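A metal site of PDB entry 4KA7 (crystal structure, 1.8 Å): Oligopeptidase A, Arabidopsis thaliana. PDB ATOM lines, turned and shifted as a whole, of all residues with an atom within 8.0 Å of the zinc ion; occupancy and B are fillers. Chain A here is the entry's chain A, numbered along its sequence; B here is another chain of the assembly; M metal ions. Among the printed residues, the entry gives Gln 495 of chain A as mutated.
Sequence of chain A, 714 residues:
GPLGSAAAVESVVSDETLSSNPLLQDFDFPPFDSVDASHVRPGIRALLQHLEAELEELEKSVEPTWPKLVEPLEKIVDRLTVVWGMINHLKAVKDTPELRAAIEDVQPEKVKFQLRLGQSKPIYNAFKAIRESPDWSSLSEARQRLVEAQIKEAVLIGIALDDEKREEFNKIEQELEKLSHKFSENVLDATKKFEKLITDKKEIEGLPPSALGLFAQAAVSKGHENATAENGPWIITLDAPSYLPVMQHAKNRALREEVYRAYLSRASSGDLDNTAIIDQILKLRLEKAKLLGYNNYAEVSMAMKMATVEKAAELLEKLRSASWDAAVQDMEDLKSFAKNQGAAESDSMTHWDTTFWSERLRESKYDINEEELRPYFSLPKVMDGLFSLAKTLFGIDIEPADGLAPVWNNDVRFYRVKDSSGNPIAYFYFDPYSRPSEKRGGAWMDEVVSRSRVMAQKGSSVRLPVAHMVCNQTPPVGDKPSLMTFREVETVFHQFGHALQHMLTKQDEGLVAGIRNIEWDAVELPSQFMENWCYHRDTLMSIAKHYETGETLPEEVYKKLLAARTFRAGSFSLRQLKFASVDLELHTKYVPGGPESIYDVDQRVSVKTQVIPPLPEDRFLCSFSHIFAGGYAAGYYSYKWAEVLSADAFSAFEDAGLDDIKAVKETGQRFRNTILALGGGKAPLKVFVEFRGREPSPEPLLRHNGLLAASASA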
ATOM      1  N   ALA A 443     -11.357  11.049  29.596  1.00  0.00           N
ATOM      2  CA  ALA A 443     -10.663  10.853  30.861  1.00  0.00           C
ATOM      3  C   ALA A 443      -9.185  11.020  30.594  1.00  0.00           C
ATOM      4  O   ALA A 443      -8.698  10.696  29.494  1.00  0.00           O
ATOM      5  CB  ALA A 443     -10.948   9.462  31.414  1.00  0.00           C
ATOM      6  N   TRP A 444      -8.456  11.541  31.585  1.00  0.00           N
ATOM      7  CA  TRP A 444      -7.044  11.814  31.405  1.00  0.00           C
ATOM      8  C   TRP A 444      -6.316  11.997  32.738  1.00  0.00           C
ATOM      9  O   TRP A 444      -6.946  12.080  33.798  1.00  0.00           O
ATOM     10  CB  TRP A 444      -6.833  13.060  30.511  1.00  0.00           C
ATOM     11  CG  TRP A 444      -7.194  14.384  31.137  1.00  0.00           C
ATOM     12  CD1 TRP A 444      -6.345  15.209  31.831  1.00  0.00           C
ATOM     13  CD2 TRP A 444      -8.466  15.043  31.119  1.00  0.00           C
ATOM     14  NE1 TRP A 444      -7.028  16.334  32.263  1.00  0.00           N
ATOM     15  CE2 TRP A 444      -8.324  16.263  31.827  1.00  0.00           C
ATOM     16  CE3 TRP A 444      -9.715  14.721  30.563  1.00  0.00           C
ATOM     17  CZ2 TRP A 444      -9.381  17.160  31.999  1.00  0.00           C
ATOM     18  CZ3 TRP A 444     -10.779  15.632  30.727  1.00  0.00           C
ATOM     19  CH2 TRP A 444     -10.599  16.835  31.436  1.00  0.00           C
ATOM     20  N   MET A 445      -5.004  12.006  32.640  1.00  0.00           N
ATOM     21  CA  MET A 445      -4.124  12.356  33.735  1.00  0.00           C
ATOM     22  C   MET A 445      -3.281  13.541  33.262  1.00  0.00           C
ATOM     23  O   MET A 445      -2.972  13.665  32.075  1.00  0.00           O
ATOM     24  CB  MET A 445      -3.248  11.146  34.087  1.00  0.00           C
ATOM     25  CG  MET A 445      -2.101  11.407  35.057  1.00  0.00           C
ATOM     26  SD  MET A 445      -0.628  11.975  34.181  1.00  0.00           S
ATOM     27  CE  MET A 445       0.404  12.446  35.567  1.00  0.00           C
ATOM     28  N   THR A 491     -11.614   2.644  33.409  1.00  0.00           N
ATOM     29  CA  THR A 491     -11.145   3.988  33.131  1.00  0.00           C
ATOM     30  C   THR A 491     -10.427   4.609  34.342  1.00  0.00           C
ATOM     31  O   THR A 491      -9.396   5.269  34.181  1.00  0.00           O
ATOM     32  CB  THR A 491     -12.301   4.879  32.656  1.00  0.00           C
ATOM     33  OG1 THR A 491     -12.823   4.321  31.433  1.00  0.00           O
ATOM     34  CG2 THR A 491     -11.834   6.289  32.386  1.00  0.00           C
ATOM     35  N   HIS A 494      -7.086   2.936  34.649  1.00  0.00           N
ATOM     36  CA  HIS A 494      -6.223   3.473  33.562  1.00  0.00           C
ATOM     37  C   HIS A 494      -5.552   4.785  33.959  1.00  0.00           C
ATOM     38  O   HIS A 494      -4.325   4.933  33.853  1.00  0.00           O
ATOM     39  CB  HIS A 494      -7.060   3.682  32.287  1.00  0.00           C
ATOM     40  CG  HIS A 494      -6.275   4.213  31.123  1.00  0.00           C
ATOM     41  ND1 HIS A 494      -5.857   3.412  30.084  1.00  0.00           N
ATOM     42  CD2 HIS A 494      -5.805   5.457  30.854  1.00  0.00           C
ATOM     43  CE1 HIS A 494      -5.184   4.133  29.201  1.00  0.00           C
ATOM     44  NE2 HIS A 494      -5.138   5.382  29.654  1.00  0.00           N
ATOM     45  N   GLN A 495      -6.353   5.755  34.386  1.00  0.00           N
ATOM     46  CA  GLN A 495      -5.777   7.057  34.739  1.00  0.00           C
ATOM     47  C   GLN A 495      -4.878   6.932  35.970  1.00  0.00           C
ATOM     48  O   GLN A 495      -3.864   7.626  36.083  1.00  0.00           O
ATOM     49  CB  GLN A 495      -6.859   8.129  34.987  1.00  0.00           C
ATOM     50  CG  GLN A 495      -7.938   8.248  33.903  1.00  0.00           C
ATOM     51  CD  GLN A 495      -7.412   8.189  32.477  1.00  0.00           C
ATOM     52  OE1 GLN A 495      -8.053   7.568  31.610  1.00  0.00           O
ATOM     53  NE2 GLN A 495      -6.280   8.803  32.218  1.00  0.00           N
ATOM     54  N   GLY A 497      -2.986   4.435  36.647  1.00  0.00           N
ATOM     55  CA  GLY A 497      -1.707   3.951  36.109  1.00  0.00           C
ATOM     56  C   GLY A 497      -0.790   5.078  35.675  1.00  0.00           C
ATOM     57  O   GLY A 497       0.412   5.063  35.987  1.00  0.00           O
ATOM     58  N   HIS A 498      -1.335   6.043  34.941  1.00  0.00           N
ATOM     59  CA  HIS A 498      -0.580   7.244  34.579  1.00  0.00           C
ATOM     60  C   HIS A 498      -0.121   7.985  35.846  1.00  0.00           C
ATOM     61  O   HIS A 498       1.049   8.386  35.945  1.00  0.00           O
ATOM     62  CB  HIS A 498      -1.426   8.219  33.753  1.00  0.00           C
ATOM     63  CG  HIS A 498      -1.661   7.797  32.345  1.00  0.00           C
ATOM     64  ND1 HIS A 498      -0.643   7.441  31.484  1.00  0.00           N
ATOM     65  CD2 HIS A 498      -2.809   7.719  31.612  1.00  0.00           C
ATOM     66  CE1 HIS A 498      -1.150   7.140  30.299  1.00  0.00           C
ATOM     67  NE2 HIS A 498      -2.463   7.298  30.355  1.00  0.00           N
ATOM     68  N   TRP A 520       6.448   8.851  23.347  1.00  0.00           N
ATOM     69  CA  TRP A 520       5.006   8.892  23.466  1.00  0.00           C
ATOM     70  C   TRP A 520       4.350   7.524  23.276  1.00  0.00           C
ATOM     71  O   TRP A 520       3.322   7.228  23.900  1.00  0.00           O
ATOM     72  CB  TRP A 520       4.401   9.912  22.484  1.00  0.00           C
ATOM     73  CG  TRP A 520       3.023  10.292  22.866  1.00  0.00           C
ATOM     74  CD1 TRP A 520       1.866   9.895  22.272  1.00  0.00           C
ATOM     75  CD2 TRP A 520       2.631  11.134  23.976  1.00  0.00           C
ATOM     76  NE1 TRP A 520       0.789  10.438  22.921  1.00  0.00           N
ATOM     77  CE2 TRP A 520       1.226  11.204  23.968  1.00  0.00           C
ATOM     78  CE3 TRP A 520       3.351  11.836  24.959  1.00  0.00           C
ATOM     79  CZ2 TRP A 520       0.499  11.952  24.909  1.00  0.00           C
ATOM     80  CZ3 TRP A 520       2.619  12.576  25.900  1.00  0.00           C
ATOM     81  CH2 TRP A 520       1.211  12.626  25.870  1.00  0.00           C
ATOM     82  N   VAL A 523       4.014   5.785  26.704  1.00  0.00           N
ATOM     83  CA  VAL A 523       3.340   6.371  27.882  1.00  0.00           C
ATOM     84  C   VAL A 523       2.038   5.667  28.257  1.00  0.00           C
ATOM     85  O   VAL A 523       1.594   5.793  29.398  1.00  0.00           O
ATOM     86  CB  VAL A 523       3.139   7.912  27.813  1.00  0.00           C
ATOM     87  CG1 VAL A 523       4.389   8.631  27.296  1.00  0.00           C
ATOM     88  CG2 VAL A 523       1.891   8.289  27.019  1.00  0.00           C
ATOM     89  N   GLU A 524       1.444   4.916  27.325  1.00  0.00           N
ATOM     90  CA  GLU A 524       0.219   4.167  27.638  1.00  0.00           C
ATOM     91  C   GLU A 524       0.499   2.777  28.192  1.00  0.00           C
ATOM     92  O   GLU A 524      -0.410   1.952  28.289  1.00  0.00           O
ATOM     93  CB  GLU A 524      -0.717   4.111  26.413  1.00  0.00           C
ATOM     94  CG  GLU A 524      -1.192   5.489  25.960  1.00  0.00           C
ATOM     95  CD  GLU A 524      -2.075   6.176  26.976  1.00  0.00           C
ATOM     96  OE1 GLU A 524      -2.729   5.481  27.796  1.00  0.00           O
ATOM     97  OE2 GLU A 524      -2.131   7.417  26.956  1.00  0.00           O
ATOM     98  N   LEU A 525       1.751   2.517  28.567  1.00  0.00           N
ATOM     99  CA  LEU A 525       2.117   1.240  29.209  1.00  0.00           C
ATOM    100  C   LEU A 525       1.518   1.102  30.616  1.00  0.00           C
ATOM    101  O   LEU A 525       0.712   0.181  30.846  1.00  0.00           O
ATOM    102  CB  LEU A 525       3.638   1.029  29.176  1.00  0.00           C
ATOM    103  CG  LEU A 525       4.389  -0.035  30.012  1.00  0.00           C
ATOM    104  CD1 LEU A 525       3.763  -1.410  30.040  1.00  0.00           C
ATOM    105  CD2 LEU A 525       5.839  -0.159  29.542  1.00  0.00           C
ATOM    106  N   PRO A 526       1.897   1.985  31.576  1.00  0.00           N
ATOM    107  CA  PRO A 526       1.413   1.707  32.935  1.00  0.00           C
ATOM    108  C   PRO A 526      -0.097   1.844  33.100  1.00  0.00           C
ATOM    109  O   PRO A 526      -0.700   1.168  33.953  1.00  0.00           O
ATOM    110  CB  PRO A 526       2.162   2.729  33.806  1.00  0.00           C
ATOM    111  CG  PRO A 526       2.478   3.860  32.867  1.00  0.00           C
ATOM    112  CD  PRO A 526       2.777   3.176  31.547  1.00  0.00           C
ATOM    113  N   SER A 527      -0.701   2.717  32.295  1.00  0.00           N
ATOM    114  CA  SER A 527      -2.149   2.915  32.331  1.00  0.00           C
ATOM    115  C   SER A 527      -2.917   1.673  31.870  1.00  0.00           C
ATOM    116  O   SER A 527      -3.783   1.166  32.581  1.00  0.00           O
ATOM    117  CB  SER A 527      -2.501   4.125  31.464  1.00  0.00           C
ATOM    118  OG  SER A 527      -1.897   3.982  30.187  1.00  0.00           O
ATOM    119  N   GLN A 528      -2.582   1.168  30.677  1.00  0.00           N
ATOM    120  CA  GLN A 528      -3.238  -0.027  30.168  1.00  0.00           C
ATOM    121  C   GLN A 528      -2.867  -1.244  30.989  1.00  0.00           C
ATOM    122  O   GLN A 528      -3.696  -2.142  31.175  1.00  0.00           O
ATOM    123  CB  GLN A 528      -2.897  -0.231  28.680  1.00  0.00           C
ATOM    124  CG  GLN A 528      -3.500   0.885  27.841  1.00  0.00           C
ATOM    125  CD  GLN A 528      -3.172   0.765  26.366  1.00  0.00           C
ATOM    126  OE1 GLN A 528      -2.004   0.881  25.950  1.00  0.00           O
ATOM    127  NE2 GLN A 528      -4.201   0.578  25.545  1.00  0.00           N
ATOM    128  N   GLU A 531      -5.301  -1.730  33.896  1.00  0.00           N
ATOM    129  CA  GLU A 531      -6.640  -2.224  33.522  1.00  0.00           C
ATOM    130  C   GLU A 531      -6.779  -3.751  33.651  1.00  0.00           C
ATOM    131  O   GLU A 531      -7.883  -4.257  33.917  1.00  0.00           O
ATOM    132  CB  GLU A 531      -7.018  -1.774  32.110  1.00  0.00           C
ATOM    133  CG  GLU A 531      -6.978  -0.265  31.887  1.00  0.00           C
ATOM    134  CD  GLU A 531      -7.547   0.129  30.537  1.00  0.00           C
ATOM    135  OE1 GLU A 531      -8.646  -0.356  30.199  1.00  0.00           O
ATOM    136  OE2 GLU A 531      -6.887   0.886  29.804  1.00  0.00           O
ATOM    137  N   HIS A 626      -7.850  13.726  20.220  1.00  0.00           N
ATOM    138  CA  HIS A 626      -6.546  13.070  20.406  1.00  0.00           C
ATOM    139  C   HIS A 626      -5.510  13.548  19.391  1.00  0.00           C
ATOM    140  O   HIS A 626      -4.352  13.763  19.737  1.00  0.00           O
ATOM    141  CB  HIS A 626      -6.673  11.556  20.246  1.00  0.00           C
ATOM    142  CG  HIS A 626      -7.167  10.843  21.464  1.00  0.00           C
ATOM    143  ND1 HIS A 626      -8.505  10.753  21.784  1.00  0.00           N
ATOM    144  CD2 HIS A 626      -6.504  10.160  22.422  1.00  0.00           C
ATOM    145  CE1 HIS A 626      -8.645  10.054  22.901  1.00  0.00           C
ATOM    146  NE2 HIS A 626      -7.446   9.686  23.306  1.00  0.00           N
ATOM    147  N   TYR A 632      -1.488  13.154  20.375  1.00  0.00           N
ATOM    148  CA  TYR A 632      -1.469  11.915  19.582  1.00  0.00           C
ATOM    149  C   TYR A 632      -1.478  12.075  18.052  1.00  0.00           C
ATOM    150  O   TYR A 632      -1.753  11.104  17.349  1.00  0.00           O
ATOM    151  CB  TYR A 632      -2.611  10.959  20.019  1.00  0.00           C
ATOM    152  CG  TYR A 632      -2.581  10.582  21.489  1.00  0.00           C
ATOM    153  CD1 TYR A 632      -3.030  11.465  22.481  1.00  0.00           C
ATOM    154  CD2 TYR A 632      -2.088   9.339  21.903  1.00  0.00           C
ATOM    155  CE1 TYR A 632      -2.993  11.120  23.830  1.00  0.00           C
ATOM    156  CE2 TYR A 632      -2.046   8.981  23.249  1.00  0.00           C
ATOM    157  CZ  TYR A 632      -2.499   9.877  24.203  1.00  0.00           C
ATOM    158  OH  TYR A 632      -2.460   9.543  25.543  1.00  0.00           O
ATOM    159  N   TYR A 639      -1.348   3.883  21.535  1.00  0.00           N
ATOM    160  CA  TYR A 639      -2.136   3.006  22.424  1.00  0.00           C
ATOM    161  C   TYR A 639      -1.823   1.519  22.169  1.00  0.00           C
ATOM    162  O   TYR A 639      -1.434   0.799  23.096  1.00  0.00           O
ATOM    163  CB  TYR A 639      -3.636   3.267  22.273  1.00  0.00           C
ATOM    164  CG  TYR A 639      -4.097   4.536  22.963  1.00  0.00           C
ATOM    165  CD1 TYR A 639      -4.307   4.571  24.344  1.00  0.00           C
ATOM    166  CD2 TYR A 639      -4.353   5.687  22.224  1.00  0.00           C
ATOM    167  CE1 TYR A 639      -4.749   5.745  24.968  1.00  0.00           C
ATOM    168  CE2 TYR A 639      -4.789   6.858  22.836  1.00  0.00           C
ATOM    169  CZ  TYR A 639      -4.972   6.880  24.210  1.00  0.00           C
ATOM    170  OH  TYR A 639      -5.406   8.041  24.801  1.00  0.00           O
ATOM    171  N   ALA B   1      -1.359  16.169  28.057  1.00  0.00           N
ATOM    172  CA  ALA B   1      -2.323  15.214  28.705  1.00  0.00           C
ATOM    173  C   ALA B   1      -2.112  13.768  28.239  1.00  0.00           C
ATOM    174  O   ALA B   1      -2.067  13.498  27.039  1.00  0.00           O
ATOM    175  CB  ALA B   1      -3.765  15.648  28.470  1.00  0.00           C
ATOM    176  N   ALA B   2      -1.992  12.864  29.199  1.00  0.00           N
ATOM    177  CA  ALA B   2      -2.002  11.440  28.934  1.00  0.00           C
ATOM    178  C   ALA B   2      -3.468  10.996  28.992  1.00  0.00           C
ATOM    179  O   ALA B   2      -4.023  10.812  30.078  1.00  0.00           O
ATOM    180  CB  ALA B   2      -1.152  10.691  29.949  1.00  0.00           C
ATOM    181  N   ALA B   3      -4.083  10.845  27.825  1.00  0.00           N
ATOM    182  CA  ALA B   3      -5.524  10.591  27.726  1.00  0.00           C
ATOM    183  C   ALA B   3      -5.885   9.121  27.988  1.00  0.00           C
ATOM    184  O   ALA B   3      -5.238   8.437  28.795  1.00  0.00           O
ATOM    185  CB  ALA B   3      -6.063  11.070  26.380  1.00  0.00           C
ATOM    186  N   ALA B   4      -6.940   8.656  27.304  1.00  0.00           N
ATOM    187  CA  ALA B   4      -7.414   7.275  27.404  1.00  0.00           C
ATOM    188  C   ALA B   4      -8.170   6.838  26.151  1.00  0.00           C
ATOM    189  O   ALA B   4      -8.580   7.676  25.334  1.00  0.00           O
ATOM    190  CB  ALA B   4      -8.279   7.099  28.635  1.00  0.00           C
HETATM  191 ZN    ZN M   1      -3.883   6.855  28.905  1.00  0.00          ZN
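A ring nitrogen (ND1) of His 498 lies close to the backbone carbonyl oxygen (O) of Val 523, at 3.5 Å. The side-chain hydroxyl (OH) of Tyr 632 lies within hydrogen-bond range of the backbone NH (N) of Ala 3 of chain B (3.1 Å). The backbone carbonyl oxygen (O) of Glu 524 sits at hydrogen-bond distance from the side-chain hydroxyl (OG) of Ser 527, 3.2 Å away. OH of Tyr 632 is in hydrogen-bond range of OE2 of Glu 524 (2.6 Å). The backbone carbonyl oxygen (O) of Glu 524 lies close to the side-chain amide oxygen (OE1) of Gln 528 (3.0 Å). The backbone NH (N) of Ala 4 of chain B sits at hydrogen-bond distance from the side-chain hydroxyl (OH) of Tyr 639, at 3.0 Å. N of Ala 4 of chain B is in hydrogen-bond range of O of Ala 443 (3.5 Å). The backbone carbonyl oxygen (O) of Ala 4 of chain B lies within hydrogen-bond range of a ring nitrogen (NE2) of His 626 (3.1 Å).
Ser 527 touches the zinc ion. CA of Ala 4 of chain B touches the zinc ion, 3.9 Å away. Six residues have an atom within 4 Å of the zinc ion: His 494, His 498, Glu 524, Ser 527, Ala 3 of chain B and Ala 4 of chain B. The nearest printed residue that does not touch the zinc ion is Ala 2 of chain B (4.1 Å).
The zinc ion is bound by NE2 of His 494. NE2 of His 498 binds the zinc ion, at 2.1 Å. The zinc ion is bound by O of Ala 3 of chain B (2.1 Å). OE1 of Glu 524 is bound to the zinc ion (2.1 Å). The zinc ion has four donor atoms within binding distance. Slightly farther from the zinc ion lies the side-chain carboxylate (OE2) of Glu 524 (2.7 Å).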
